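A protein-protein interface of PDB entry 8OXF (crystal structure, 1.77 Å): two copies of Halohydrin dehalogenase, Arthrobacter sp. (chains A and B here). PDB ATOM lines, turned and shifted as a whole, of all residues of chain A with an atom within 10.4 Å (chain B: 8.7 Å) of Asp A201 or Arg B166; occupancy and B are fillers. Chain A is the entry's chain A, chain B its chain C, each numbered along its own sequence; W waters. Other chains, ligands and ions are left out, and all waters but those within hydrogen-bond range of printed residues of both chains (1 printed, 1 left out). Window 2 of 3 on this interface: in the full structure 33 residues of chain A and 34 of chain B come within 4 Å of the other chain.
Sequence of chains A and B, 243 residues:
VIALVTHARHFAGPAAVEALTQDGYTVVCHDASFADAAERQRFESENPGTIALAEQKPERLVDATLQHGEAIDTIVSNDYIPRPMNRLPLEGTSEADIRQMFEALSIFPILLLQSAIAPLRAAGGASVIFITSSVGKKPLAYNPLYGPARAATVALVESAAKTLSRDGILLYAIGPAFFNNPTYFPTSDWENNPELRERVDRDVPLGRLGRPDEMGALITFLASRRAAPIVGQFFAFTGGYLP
Asp A201 touches just one residue of chain B: Arg B166 (2.8 Å). Of the printed residues of chain A, Lys B162 touches Pro A205, Gly A240 and Tyr A241. Of chain A, only Pro A205 and Leu A206 come within 4 Å of Ser B165. Arg B166 touches just these residues of chain A: Val A200, Asp A201, Val A204, Pro A205, Leu A206 and Gly A207. No residue of chain A comes within 4 Å of Asp B167. Of the printed residues of chain A, Val B231 touches Gly A239 and Gly A240. The nearest residue of chain B that does not touch Asp A201 is Lys B162 (7.7 Å).
Water W1 lies within hydrogen-bond range of the backbone carbonyl oxygen (O) of Tyr A241 (3.0 Å) and the side-chain amino group (NZ) of Lys B162 (3.5 Å).
The side-chain carboxylate (OD1) of Asp A201 lies within salt-bridge range of the guanidinium group (NH1) of Arg B166, 2.8 Å away. O of Val A204 sits at hydrogen-bond distance from NH2 of Arg B166, at 2.9 Å. The backbone carbonyl oxygen (O) of Pro A205 lies within hydrogen-bond range of the guanidinium group (NE) of Arg B166 (2.7 Å). NZ of Lys B162 sits at hydrogen-bond distance from O of Gly A240 (2.7 Å).
No position is printed for both chains.
Printed residues of chain A that touch a printed residue of chain B: Val A200, Asp A201, Val A204, Pro A205, Leu A206, Gly A207, Gly A239, Gly A240 and Tyr A241. Hydrophobic or aromatic side chains of chain A within 4 Å of the printed part of chain B: Pro A205. Hydrophobic or aromatic side chains of chain B that line the printed part of chain A: Val B231. Among the printed residues, 14 pairs touch across the chains.
Val A200 touches Arg B166 (O to NH2, 3.98 Å). CB of Pro A205 touches O of Ala B161, at 3.6 Å. Pro A205 touches Lys B162 (CB to O, 3.6 Å). Ser B165 touches Pro A205 (CB to CB, 3.6 Å). Leu A206 touches Ser B165 (N to CB, 3.9 Å). Leu A206 touches Arg B166 (C to NE, 3.96 Å). CA of Gly A207 touches NE of Arg B166, 3.5 Å away. C of Gly A239 touches CG1 of Val B231, 3.8 Å away. Gly A240 touches Val B231. Tyr A241 touches Lys B162.
The backbone carbonyl oxygen of Gly A239 is in hydrogen-bond range of the backbone NH of Leu A206 (3.0 Å). The backbone NH (N) of Gly A240 lies close to the side-chain hydroxyl (OG1) of Thr A238 (3.5 Å). N of Tyr A241 is in hydrogen-bond range of OG1 of Thr A238. The side-chain hydroxyl (OG) of Ser B165 is in hydrogen-bond range of the backbone carbonyl oxygen (O) of Ala B161.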
ATOM      1  N   PHE A 178      22.051 -13.777  -8.611  1.00  0.00           N
ATOM      2  CA  PHE A 178      21.581 -14.432  -9.826  1.00  0.00           C
ATOM      3  C   PHE A 178      22.521 -15.568 -10.219  1.00  0.00           C
ATOM      4  O   PHE A 178      22.856 -15.757 -11.390  1.00  0.00           O
ATOM      5  CB  PHE A 178      21.430 -13.409 -10.949  1.00  0.00           C
ATOM      6  CG  PHE A 178      20.444 -12.343 -10.629  1.00  0.00           C
ATOM      7  CD1 PHE A 178      19.084 -12.626 -10.613  1.00  0.00           C
ATOM      8  CD2 PHE A 178      20.869 -11.081 -10.263  1.00  0.00           C
ATOM      9  CE1 PHE A 178      18.166 -11.646 -10.291  1.00  0.00           C
ATOM     10  CE2 PHE A 178      19.957 -10.104  -9.934  1.00  0.00           C
ATOM     11  CZ  PHE A 178      18.599 -10.386  -9.955  1.00  0.00           C
ATOM     12  N   TRP A 190      14.232 -21.152 -12.611  1.00  0.00           N
ATOM     13  CA  TRP A 190      14.318 -20.497 -13.911  1.00  0.00           C
ATOM     14  C   TRP A 190      13.176 -20.938 -14.822  1.00  0.00           C
ATOM     15  O   TRP A 190      12.550 -20.114 -15.494  1.00  0.00           O
ATOM     16  CB  TRP A 190      15.680 -20.783 -14.554  1.00  0.00           C
ATOM     17  CG  TRP A 190      15.842 -20.122 -15.898  1.00  0.00           C
ATOM     18  CD1 TRP A 190      15.668 -20.694 -17.125  1.00  0.00           C
ATOM     19  CD2 TRP A 190      16.185 -18.747 -16.141  1.00  0.00           C
ATOM     20  NE1 TRP A 190      15.887 -19.766 -18.116  1.00  0.00           N
ATOM     21  CE2 TRP A 190      16.197 -18.560 -17.540  1.00  0.00           C
ATOM     22  CE3 TRP A 190      16.475 -17.659 -15.312  1.00  0.00           C
ATOM     23  CZ2 TRP A 190      16.506 -17.328 -18.130  1.00  0.00           C
ATOM     24  CZ3 TRP A 190      16.781 -16.432 -15.903  1.00  0.00           C
ATOM     25  CH2 TRP A 190      16.797 -16.281 -17.298  1.00  0.00           C
ATOM     26  N   ASN A 193       9.454 -19.953 -12.942  1.00  0.00           N
ATOM     27  CA  ASN A 193       9.174 -18.601 -12.463  1.00  0.00           C
ATOM     28  C   ASN A 193       9.412 -17.617 -13.599  1.00  0.00           C
ATOM     29  O   ASN A 193      10.520 -17.079 -13.741  1.00  0.00           O
ATOM     30  CB  ASN A 193      10.044 -18.274 -11.249  1.00  0.00           C
ATOM     31  CG  ASN A 193       9.701 -16.940 -10.613  1.00  0.00           C
ATOM     32  OD1 ASN A 193       8.982 -16.123 -11.196  1.00  0.00           O
ATOM     33  ND2 ASN A 193      10.217 -16.712  -9.409  1.00  0.00           N
ATOM     34  N   PRO A 194       8.399 -17.333 -14.420  1.00  0.00           N
ATOM     35  CA  PRO A 194       8.585 -16.320 -15.471  1.00  0.00           C
ATOM     36  C   PRO A 194       8.941 -14.941 -14.929  1.00  0.00           C
ATOM     37  O   PRO A 194       9.526 -14.146 -15.671  1.00  0.00           O
ATOM     38  CB  PRO A 194       7.235 -16.315 -16.206  1.00  0.00           C
ATOM     39  CG  PRO A 194       6.255 -16.823 -15.213  1.00  0.00           C
ATOM     40  CD  PRO A 194       7.007 -17.809 -14.343  1.00  0.00           C
ATOM     41  N   GLU A 195       8.621 -14.630 -13.667  1.00  0.00           N
ATOM     42  CA  GLU A 195       9.077 -13.365 -13.091  1.00  0.00           C
ATOM     43  C   GLU A 195      10.589 -13.336 -12.948  1.00  0.00           C
ATOM     44  O   GLU A 195      11.216 -12.286 -13.126  1.00  0.00           O
ATOM     45  CB  GLU A 195       8.426 -13.112 -11.735  1.00  0.00           C
ATOM     46  CG  GLU A 195       8.749 -11.732 -11.144  1.00  0.00           C
ATOM     47  CD  GLU A 195       8.669 -10.604 -12.166  1.00  0.00           C
ATOM     48  OE1 GLU A 195       7.563 -10.380 -12.716  1.00  0.00           O
ATOM     49  OE2 GLU A 195       9.709  -9.936 -12.423  1.00  0.00           O
ATOM     50  N   LEU A 196      11.192 -14.473 -12.616  1.00  0.00           N
ATOM     51  CA  LEU A 196      12.644 -14.500 -12.467  1.00  0.00           C
ATOM     52  C   LEU A 196      13.335 -14.224 -13.797  1.00  0.00           C
ATOM     53  O   LEU A 196      14.342 -13.506 -13.844  1.00  0.00           O
ATOM     54  CB  LEU A 196      13.099 -15.847 -11.900  1.00  0.00           C
ATOM     55  CG  LEU A 196      14.613 -16.005 -11.805  1.00  0.00           C
ATOM     56  CD1 LEU A 196      15.153 -14.934 -10.885  1.00  0.00           C
ATOM     57  CD2 LEU A 196      15.007 -17.394 -11.312  1.00  0.00           C
ATOM     58  N   ARG A 197      12.797 -14.772 -14.890  1.00  0.00           N
ATOM     59  CA  ARG A 197      13.414 -14.571 -16.195  1.00  0.00           C
ATOM     60  C   ARG A 197      13.288 -13.119 -16.644  1.00  0.00           C
ATOM     61  O   ARG A 197      14.233 -12.555 -17.211  1.00  0.00           O
ATOM     62  CB  ARG A 197      12.792 -15.525 -17.218  1.00  0.00           C
ATOM     63  CG  ARG A 197      12.864 -17.005 -16.812  1.00  0.00           C
ATOM     64  CD  ARG A 197      12.537 -17.954 -17.981  1.00  0.00           C
ATOM     65  NE  ARG A 197      11.150 -17.817 -18.408  1.00  0.00           N
ATOM     66  CZ  ARG A 197      10.129 -18.479 -17.874  1.00  0.00           C
ATOM     67  NH1 ARG A 197      10.309 -19.381 -16.915  1.00  0.00           N
ATOM     68  NH2 ARG A 197       8.895 -18.224 -18.303  1.00  0.00           N
ATOM     69  N   GLU A 198      12.133 -12.498 -16.388  1.00  0.00           N
ATOM     70  CA  GLU A 198      11.963 -11.077 -16.692  1.00  0.00           C
ATOM     71  C   GLU A 198      12.885 -10.218 -15.841  1.00  0.00           C
ATOM     72  O   GLU A 198      13.504  -9.272 -16.342  1.00  0.00           O
ATOM     73  CB  GLU A 198      10.511 -10.646 -16.479  1.00  0.00           C
ATOM     74  CG  GLU A 198       9.575 -10.999 -17.630  1.00  0.00           C
ATOM     75  CD  GLU A 198       8.687  -9.826 -18.040  1.00  0.00           C
ATOM     76  OE1 GLU A 198       7.481 -10.040 -18.322  1.00  0.00           O
ATOM     77  OE2 GLU A 198       9.204  -8.685 -18.087  1.00  0.00           O
ATOM     78  N   ARG A 199      12.972 -10.526 -14.545  1.00  0.00           N
ATOM     79  CA  ARG A 199      13.840  -9.764 -13.657  1.00  0.00           C
ATOM     80  C   ARG A 199      15.299  -9.861 -14.113  1.00  0.00           C
ATOM     81  O   ARG A 199      16.022  -8.853 -14.134  1.00  0.00           O
ATOM     82  CB  ARG A 199      13.639 -10.267 -12.226  1.00  0.00           C
ATOM     83  CG  ARG A 199      14.540  -9.681 -11.166  1.00  0.00           C
ATOM     84  CD  ARG A 199      14.245 -10.333  -9.811  1.00  0.00           C
ATOM     85  NE  ARG A 199      15.321 -10.097  -8.855  1.00  0.00           N
ATOM     86  CZ  ARG A 199      15.564 -10.848  -7.788  1.00  0.00           C
ATOM     87  NH1 ARG A 199      14.849 -11.931  -7.523  1.00  0.00           N
ATOM     88  NH2 ARG A 199      16.562 -10.513  -6.975  1.00  0.00           N
ATOM     89  N   VAL A 200      15.729 -11.054 -14.536  1.00  0.00           N
ATOM     90  CA  VAL A 200      17.089 -11.241 -15.046  1.00  0.00           C
ATOM     91  C   VAL A 200      17.297 -10.479 -16.362  1.00  0.00           C
ATOM     92  O   VAL A 200      18.323  -9.811 -16.551  1.00  0.00           O
ATOM     93  CB  VAL A 200      17.395 -12.747 -15.171  1.00  0.00           C
ATOM     94  CG1 VAL A 200      18.677 -12.987 -15.952  1.00  0.00           C
ATOM     95  CG2 VAL A 200      17.514 -13.376 -13.775  1.00  0.00           C
ATOM     96  N   ASP A 201      16.334 -10.547 -17.294  1.00  0.00           N
ATOM     97  CA  ASP A 201      16.462  -9.733 -18.499  1.00  0.00           C
ATOM     98  C   ASP A 201      16.642  -8.263 -18.147  1.00  0.00           C
ATOM     99  O   ASP A 201      17.471  -7.569 -18.744  1.00  0.00           O
ATOM    100  CB  ASP A 201      15.241  -9.923 -19.408  1.00  0.00           C
ATOM    101  CG  ASP A 201      15.280  -9.029 -20.644  1.00  0.00           C
ATOM    102  OD1 ASP A 201      16.244  -9.119 -21.430  1.00  0.00           O
ATOM    103  OD2 ASP A 201      14.332  -8.232 -20.834  1.00  0.00           O
ATOM    104  N   ARG A 202      15.910  -7.782 -17.142  1.00  0.00           N
ATOM    105  CA  ARG A 202      15.939  -6.355 -16.838  1.00  0.00           C
ATOM    106  C   ARG A 202      17.219  -5.951 -16.112  1.00  0.00           C
ATOM    107  O   ARG A 202      17.840  -4.947 -16.474  1.00  0.00           O
ATOM    108  CB  ARG A 202      14.716  -5.974 -16.009  1.00  0.00           C
ATOM    109  CG  ARG A 202      14.678  -4.508 -15.620  1.00  0.00           C
ATOM    110  CD  ARG A 202      13.510  -4.226 -14.680  1.00  0.00           C
ATOM    111  NE  ARG A 202      12.634  -5.386 -14.541  1.00  0.00           N
ATOM    112  CZ  ARG A 202      12.372  -6.008 -13.395  1.00  0.00           C
ATOM    113  NH1 ARG A 202      12.986  -5.674 -12.269  1.00  0.00           N
ATOM    114  NH2 ARG A 202      11.480  -7.000 -13.385  1.00  0.00           N
ATOM    115  N   ASP A 203      17.645  -6.728 -15.112  1.00  0.00           N
ATOM    116  CA  ASP A 203      18.671  -6.298 -14.162  1.00  0.00           C
ATOM    117  C   ASP A 203      20.051  -6.934 -14.326  1.00  0.00           C
ATOM    118  O   ASP A 203      20.991  -6.490 -13.655  1.00  0.00           O
ATOM    119  CB  ASP A 203      18.196  -6.572 -12.731  1.00  0.00           C
ATOM    120  CG  ASP A 203      16.950  -5.815 -12.382  1.00  0.00           C
ATOM    121  OD1 ASP A 203      16.709  -4.750 -13.003  1.00  0.00           O
ATOM    122  OD2 ASP A 203      16.204  -6.282 -11.496  1.00  0.00           O
ATOM    123  N   VAL A 204      20.198  -7.979 -15.132  1.00  0.00           N
ATOM    124  CA  VAL A 204      21.470  -8.696 -15.234  1.00  0.00           C
ATOM    125  C   VAL A 204      22.033  -8.508 -16.639  1.00  0.00           C
ATOM    126  O   VAL A 204      21.580  -9.169 -17.590  1.00  0.00           O
ATOM    127  CB  VAL A 204      21.321 -10.192 -14.908  1.00  0.00           C
ATOM    128  CG1 VAL A 204      22.693 -10.883 -14.981  1.00  0.00           C
ATOM    129  CG2 VAL A 204      20.636 -10.412 -13.552  1.00  0.00           C
ATOM    130  N   PRO A 205      23.015  -7.615 -16.808  1.00  0.00           N
ATOM    131  CA  PRO A 205      23.607  -7.393 -18.134  1.00  0.00           C
ATOM    132  C   PRO A 205      23.952  -8.663 -18.881  1.00  0.00           C
ATOM    133  O   PRO A 205      23.682  -8.757 -20.086  1.00  0.00           O
ATOM    134  CB  PRO A 205      24.867  -6.577 -17.798  1.00  0.00           C
ATOM    135  CG  PRO A 205      24.486  -5.805 -16.578  1.00  0.00           C
ATOM    136  CD  PRO A 205      23.671  -6.813 -15.766  1.00  0.00           C
ATOM    137  N   LEU A 206      24.525  -9.660 -18.193  1.00  0.00           N
ATOM    138  CA  LEU A 206      24.848 -10.914 -18.859  1.00  0.00           C
ATOM    139  C   LEU A 206      23.599 -11.566 -19.448  1.00  0.00           C
ATOM    140  O   LEU A 206      23.694 -12.306 -20.430  1.00  0.00           O
ATOM    141  CB  LEU A 206      25.542 -11.874 -17.886  1.00  0.00           C
ATOM    142  CG  LEU A 206      26.494 -12.908 -18.496  1.00  0.00           C
ATOM    143  CD1 LEU A 206      27.529 -12.247 -19.391  1.00  0.00           C
ATOM    144  CD2 LEU A 206      27.173 -13.753 -17.413  1.00  0.00           C
ATOM    145  N   GLY A 207      22.434 -11.315 -18.863  1.00  0.00           N
ATOM    146  CA  GLY A 207      21.202 -11.829 -19.409  1.00  0.00           C
ATOM    147  C   GLY A 207      20.838 -13.220 -18.953  1.00  0.00           C
ATOM    148  O   GLY A 207      19.845 -13.767 -19.442  1.00  0.00           O
ATOM    149  N   ARG A 208      21.597 -13.806 -18.026  1.00  0.00           N
ATOM    150  CA  ARG A 208      21.367 -15.184 -17.622  1.00  0.00           C
ATOM    151  C   ARG A 208      21.905 -15.377 -16.213  1.00  0.00           C
ATOM    152  O   ARG A 208      22.675 -14.557 -15.709  1.00  0.00           O
ATOM    153  CB  ARG A 208      22.023 -16.172 -18.597  1.00  0.00           C
ATOM    154  CG  ARG A 208      23.529 -15.961 -18.772  1.00  0.00           C
ATOM    155  CD  ARG A 208      24.195 -17.164 -19.404  1.00  0.00           C
ATOM    156  NE  ARG A 208      25.619 -16.941 -19.619  1.00  0.00           N
ATOM    157  CZ  ARG A 208      26.552 -17.282 -18.741  1.00  0.00           C
ATOM    158  NH1 ARG A 208      26.233 -17.797 -17.567  1.00  0.00           N
ATOM    159  NH2 ARG A 208      27.835 -17.098 -19.051  1.00  0.00           N
ATOM    160  N   LEU A 209      21.492 -16.475 -15.585  1.00  0.00           N
ATOM    161  CA  LEU A 209      22.082 -16.837 -14.300  1.00  0.00           C
ATOM    162  C   LEU A 209      23.512 -17.306 -14.507  1.00  0.00           C
ATOM    163  O   LEU A 209      23.848 -17.904 -15.536  1.00  0.00           O
ATOM    164  CB  LEU A 209      21.277 -17.947 -13.624  1.00  0.00           C
ATOM    165  CG  LEU A 209      19.793 -17.694 -13.365  1.00  0.00           C
ATOM    166  CD1 LEU A 209      19.214 -18.882 -12.605  1.00  0.00           C
ATOM    167  CD2 LEU A 209      19.583 -16.419 -12.582  1.00  0.00           C
ATOM    168  N   THR A 238      27.881 -11.531 -10.304  1.00  0.00           N
ATOM    169  CA  THR A 238      26.515 -11.060 -10.486  1.00  0.00           C
ATOM    170  C   THR A 238      26.139 -10.831 -11.947  1.00  0.00           C
ATOM    171  O   THR A 238      25.103 -10.193 -12.205  1.00  0.00           O
ATOM    172  CB  THR A 238      26.270  -9.742  -9.735  1.00  0.00           C
ATOM    173  OG1 THR A 238      26.975  -8.687 -10.406  1.00  0.00           O
ATOM    174  CG2 THR A 238      26.711  -9.822  -8.246  1.00  0.00           C
ATOM    175  N   GLY A 239      26.954 -11.266 -12.906  1.00  0.00           N
ATOM    176  CA  GLY A 239      26.658 -10.983 -14.301  1.00  0.00           C
ATOM    177  C   GLY A 239      26.578  -9.507 -14.637  1.00  0.00           C
ATOM    178  O   GLY A 239      25.889  -9.133 -15.598  1.00  0.00           O
ATOM    179  N   GLY A 240      27.250  -8.646 -13.861  1.00  0.00           N
ATOM    180  CA  GLY A 240      27.198  -7.214 -14.088  1.00  0.00           C
ATOM    181  C   GLY A 240      26.085  -6.480 -13.369  1.00  0.00           C
ATOM    182  O   GLY A 240      25.903  -5.276 -13.598  1.00  0.00           O
ATOM    183  N   TYR A 241      25.320  -7.166 -12.520  1.00  0.00           N
ATOM    184  CA  TYR A 241      24.306  -6.492 -11.710  1.00  0.00           C
ATOM    185  C   TYR A 241      24.941  -5.543 -10.697  1.00  0.00           C
ATOM    186  O   TYR A 241      24.436  -4.432 -10.468  1.00  0.00           O
ATOM    187  CB  TYR A 241      23.448  -7.544 -11.020  1.00  0.00           C
ATOM    188  CG  TYR A 241      22.497  -7.044  -9.971  1.00  0.00           C
ATOM    189  CD1 TYR A 241      21.409  -6.242 -10.302  1.00  0.00           C
ATOM    190  CD2 TYR A 241      22.649  -7.428  -8.647  1.00  0.00           C
ATOM    191  CE1 TYR A 241      20.533  -5.808  -9.324  1.00  0.00           C
ATOM    192  CE2 TYR A 241      21.773  -7.007  -7.670  1.00  0.00           C
ATOM    193  CZ  TYR A 241      20.720  -6.197  -8.010  1.00  0.00           C
ATOM    194  OH  TYR A 241      19.858  -5.783  -7.021  1.00  0.00           O
ATOM    195  N   ARG B 121      31.139  -7.633 -31.368  1.00  0.00           N
ATOM    196  CA  ARG B 121      29.795  -8.194 -31.301  1.00  0.00           C
ATOM    197  C   ARG B 121      29.551  -9.187 -32.433  1.00  0.00           C
ATOM    198  O   ARG B 121      28.949 -10.248 -32.214  1.00  0.00           O
ATOM    199  CB  ARG B 121      28.762  -7.066 -31.320  1.00  0.00           C
ATOM    200  CG  ARG B 121      27.323  -7.530 -31.523  1.00  0.00           C
ATOM    201  CD  ARG B 121      26.470  -6.354 -31.949  1.00  0.00           C
ATOM    202  NE  ARG B 121      26.323  -5.446 -30.821  1.00  0.00           N
ATOM    203  CZ  ARG B 121      26.590  -4.150 -30.864  1.00  0.00           C
ATOM    204  NH1 ARG B 121      26.973  -3.558 -31.988  1.00  0.00           N
ATOM    205  NH2 ARG B 121      26.478  -3.431 -29.751  1.00  0.00           N
ATOM    206  N   GLY B 124      30.628 -12.589 -31.820  1.00  0.00           N
ATOM    207  CA  GLY B 124      29.939 -13.286 -30.752  1.00  0.00           C
ATOM    208  C   GLY B 124      30.476 -13.014 -29.367  1.00  0.00           C
ATOM    209  O   GLY B 124      30.124 -13.740 -28.429  1.00  0.00           O
ATOM    210  N   GLY B 125      31.316 -12.002 -29.211  1.00  0.00           N
ATOM    211  CA  GLY B 125      31.851 -11.623 -27.919  1.00  0.00           C
ATOM    212  C   GLY B 125      33.370 -11.555 -27.916  1.00  0.00           C
ATOM    213  O   GLY B 125      34.047 -11.921 -28.875  1.00  0.00           O
ATOM    214  N   ALA B 160      29.747   0.950 -19.155  1.00  0.00           N
ATOM    215  CA  ALA B 160      29.649   0.276 -20.452  1.00  0.00           C
ATOM    216  C   ALA B 160      29.312  -1.206 -20.308  1.00  0.00           C
ATOM    217  O   ALA B 160      28.630  -1.778 -21.171  1.00  0.00           O
ATOM    218  CB  ALA B 160      30.953   0.443 -21.226  1.00  0.00           C
ATOM    219  N   ALA B 161      29.781  -1.853 -19.236  1.00  0.00           N
ATOM    220  CA  ALA B 161      29.463  -3.262 -19.064  1.00  0.00           C
ATOM    221  C   ALA B 161      27.964  -3.500 -18.909  1.00  0.00           C
ATOM    222  O   ALA B 161      27.505  -4.597 -19.225  1.00  0.00           O
ATOM    223  CB  ALA B 161      30.209  -3.844 -17.854  1.00  0.00           C
ATOM    224  N   LYS B 162      27.195  -2.493 -18.461  1.00  0.00           N
ATOM    225  CA  LYS B 162      25.754  -2.664 -18.285  1.00  0.00           C
ATOM    226  C   LYS B 162      25.055  -2.973 -19.609  1.00  0.00           C
ATOM    227  O   LYS B 162      23.990  -3.602 -19.616  1.00  0.00           O
ATOM    228  CB  LYS B 162      25.112  -1.418 -17.646  1.00  0.00           C
ATOM    229  CG  LYS B 162      25.719  -0.980 -16.306  1.00  0.00           C
ATOM    230  CD  LYS B 162      25.800  -2.135 -15.303  1.00  0.00           C
ATOM    231  CE  LYS B 162      26.179  -1.631 -13.919  1.00  0.00           C
ATOM    232  NZ  LYS B 162      26.659  -2.728 -13.022  1.00  0.00           N
ATOM    233  N   THR B 163      25.624  -2.543 -20.725  1.00  0.00           N
ATOM    234  CA  THR B 163      25.050  -2.843 -22.031  1.00  0.00           C
ATOM    235  C   THR B 163      25.888  -3.837 -22.822  1.00  0.00           C
ATOM    236  O   THR B 163      25.333  -4.773 -23.409  1.00  0.00           O
ATOM    237  CB  THR B 163      24.883  -1.564 -22.854  1.00  0.00           C
ATOM    238  OG1 THR B 163      26.087  -0.786 -22.784  1.00  0.00           O
ATOM    239  CG2 THR B 163      23.759  -0.734 -22.280  1.00  0.00           C
ATOM    240  N   LEU B 164      27.215  -3.682 -22.834  1.00  0.00           N
ATOM    241  CA  LEU B 164      28.034  -4.534 -23.697  1.00  0.00           C
ATOM    242  C   LEU B 164      28.010  -6.000 -23.283  1.00  0.00           C
ATOM    243  O   LEU B 164      28.247  -6.862 -24.141  1.00  0.00           O
ATOM    244  CB  LEU B 164      29.476  -4.026 -23.741  1.00  0.00           C
ATOM    245  CG  LEU B 164      29.572  -2.645 -24.399  1.00  0.00           C
ATOM    246  CD1 LEU B 164      30.997  -2.077 -24.450  1.00  0.00           C
ATOM    247  CD2 LEU B 164      28.979  -2.664 -25.798  1.00  0.00           C
ATOM    248  N   SER B 165      27.701  -6.305 -22.009  1.00  0.00           N
ATOM    249  CA  SER B 165      27.729  -7.694 -21.540  1.00  0.00           C
ATOM    250  C   SER B 165      26.723  -8.559 -22.294  1.00  0.00           C
ATOM    251  O   SER B 165      26.974  -9.744 -22.552  1.00  0.00           O
ATOM    252  CB  SER B 165      27.423  -7.765 -20.039  1.00  0.00           C
ATOM    253  OG  SER B 165      28.433  -7.140 -19.263  1.00  0.00           O
ATOM    254  N   ARG B 166      25.557  -7.996 -22.604  1.00  0.00           N
ATOM    255  CA  ARG B 166      24.531  -8.739 -23.330  1.00  0.00           C
ATOM    256  C   ARG B 166      25.026  -9.172 -24.704  1.00  0.00           C
ATOM    257  O   ARG B 166      24.530 -10.169 -25.240  1.00  0.00           O
ATOM    258  CB  ARG B 166      23.254  -7.896 -23.436  1.00  0.00           C
ATOM    259  CG  ARG B 166      22.023  -8.674 -23.841  1.00  0.00           C
ATOM    260  CD  ARG B 166      21.623  -9.665 -22.737  1.00  0.00           C
ATOM    261  NE  ARG B 166      21.328  -9.023 -21.458  1.00  0.00           N
ATOM    262  CZ  ARG B 166      20.115  -8.725 -21.012  1.00  0.00           C
ATOM    263  NH1 ARG B 166      19.037  -8.924 -21.757  1.00  0.00           N
ATOM    264  NH2 ARG B 166      19.982  -8.212 -19.791  1.00  0.00           N
ATOM    265  N   ASP B 167      26.019  -8.467 -25.265  1.00  0.00           N
ATOM    266  CA  ASP B 167      26.626  -8.847 -26.535  1.00  0.00           C
ATOM    267  C   ASP B 167      27.739  -9.873 -26.375  1.00  0.00           C
ATOM    268  O   ASP B 167      28.384 -10.221 -27.367  1.00  0.00           O
ATOM    269  CB  ASP B 167      27.196  -7.616 -27.253  1.00  0.00           C
ATOM    270  CG  ASP B 167      26.125  -6.615 -27.645  1.00  0.00           C
ATOM    271  OD1 ASP B 167      25.126  -7.023 -28.270  1.00  0.00           O
ATOM    272  OD2 ASP B 167      26.288  -5.415 -27.344  1.00  0.00           O
ATOM    273  N   GLY B 168      27.981 -10.361 -25.159  1.00  0.00           N
ATOM    274  CA  GLY B 168      29.132 -11.189 -24.921  1.00  0.00           C
ATOM    275  C   GLY B 168      30.447 -10.444 -24.889  1.00  0.00           C
ATOM    276  O   GLY B 168      31.506 -11.090 -24.884  1.00  0.00           O
ATOM    277  N   ILE B 169      30.422  -9.114 -24.846  1.00  0.00           N
ATOM    278  CA  ILE B 169      31.641  -8.308 -24.784  1.00  0.00           C
ATOM    279  C   ILE B 169      31.867  -7.999 -23.312  1.00  0.00           C
ATOM    280  O   ILE B 169      31.115  -7.224 -22.709  1.00  0.00           O
ATOM    281  CB  ILE B 169      31.542  -7.026 -25.624  1.00  0.00           C
ATOM    282  CG1 ILE B 169      31.182  -7.364 -27.082  1.00  0.00           C
ATOM    283  CG2 ILE B 169      32.881  -6.228 -25.536  1.00  0.00           C
ATOM    284  CD1 ILE B 169      30.705  -6.141 -27.941  1.00  0.00           C
ATOM    285  N   LEU B 170      32.877  -8.639 -22.723  1.00  0.00           N
ATOM    286  CA  LEU B 170      33.080  -8.620 -21.280  1.00  0.00           C
ATOM    287  C   LEU B 170      34.192  -7.631 -20.934  1.00  0.00           C
ATOM    288  O   LEU B 170      35.343  -7.811 -21.351  1.00  0.00           O
ATOM    289  CB  LEU B 170      33.395 -10.024 -20.754  1.00  0.00           C
ATOM    290  CG  LEU B 170      32.511 -11.173 -21.285  1.00  0.00           C
ATOM    291  CD1 LEU B 170      32.960 -12.544 -20.736  1.00  0.00           C
ATOM    292  CD2 LEU B 170      31.055 -10.919 -20.951  1.00  0.00           C
ATOM    293  N   VAL B 231      32.018 -10.093 -14.717  1.00  0.00           N
ATOM    294  CA  VAL B 231      32.197  -9.016 -15.686  1.00  0.00           C
ATOM    295  C   VAL B 231      31.842  -7.664 -15.062  1.00  0.00           C
ATOM    296  O   VAL B 231      30.991  -7.566 -14.174  1.00  0.00           O
ATOM    297  CB  VAL B 231      31.339  -9.281 -16.938  1.00  0.00           C
ATOM    298  CG1 VAL B 231      29.882  -9.479 -16.536  1.00  0.00           C
ATOM    299  CG2 VAL B 231      31.447  -8.141 -17.947  1.00  0.00           C
HETATM  300  O   HOH W   1      23.214  -2.673 -12.578  1.00  0.00           O
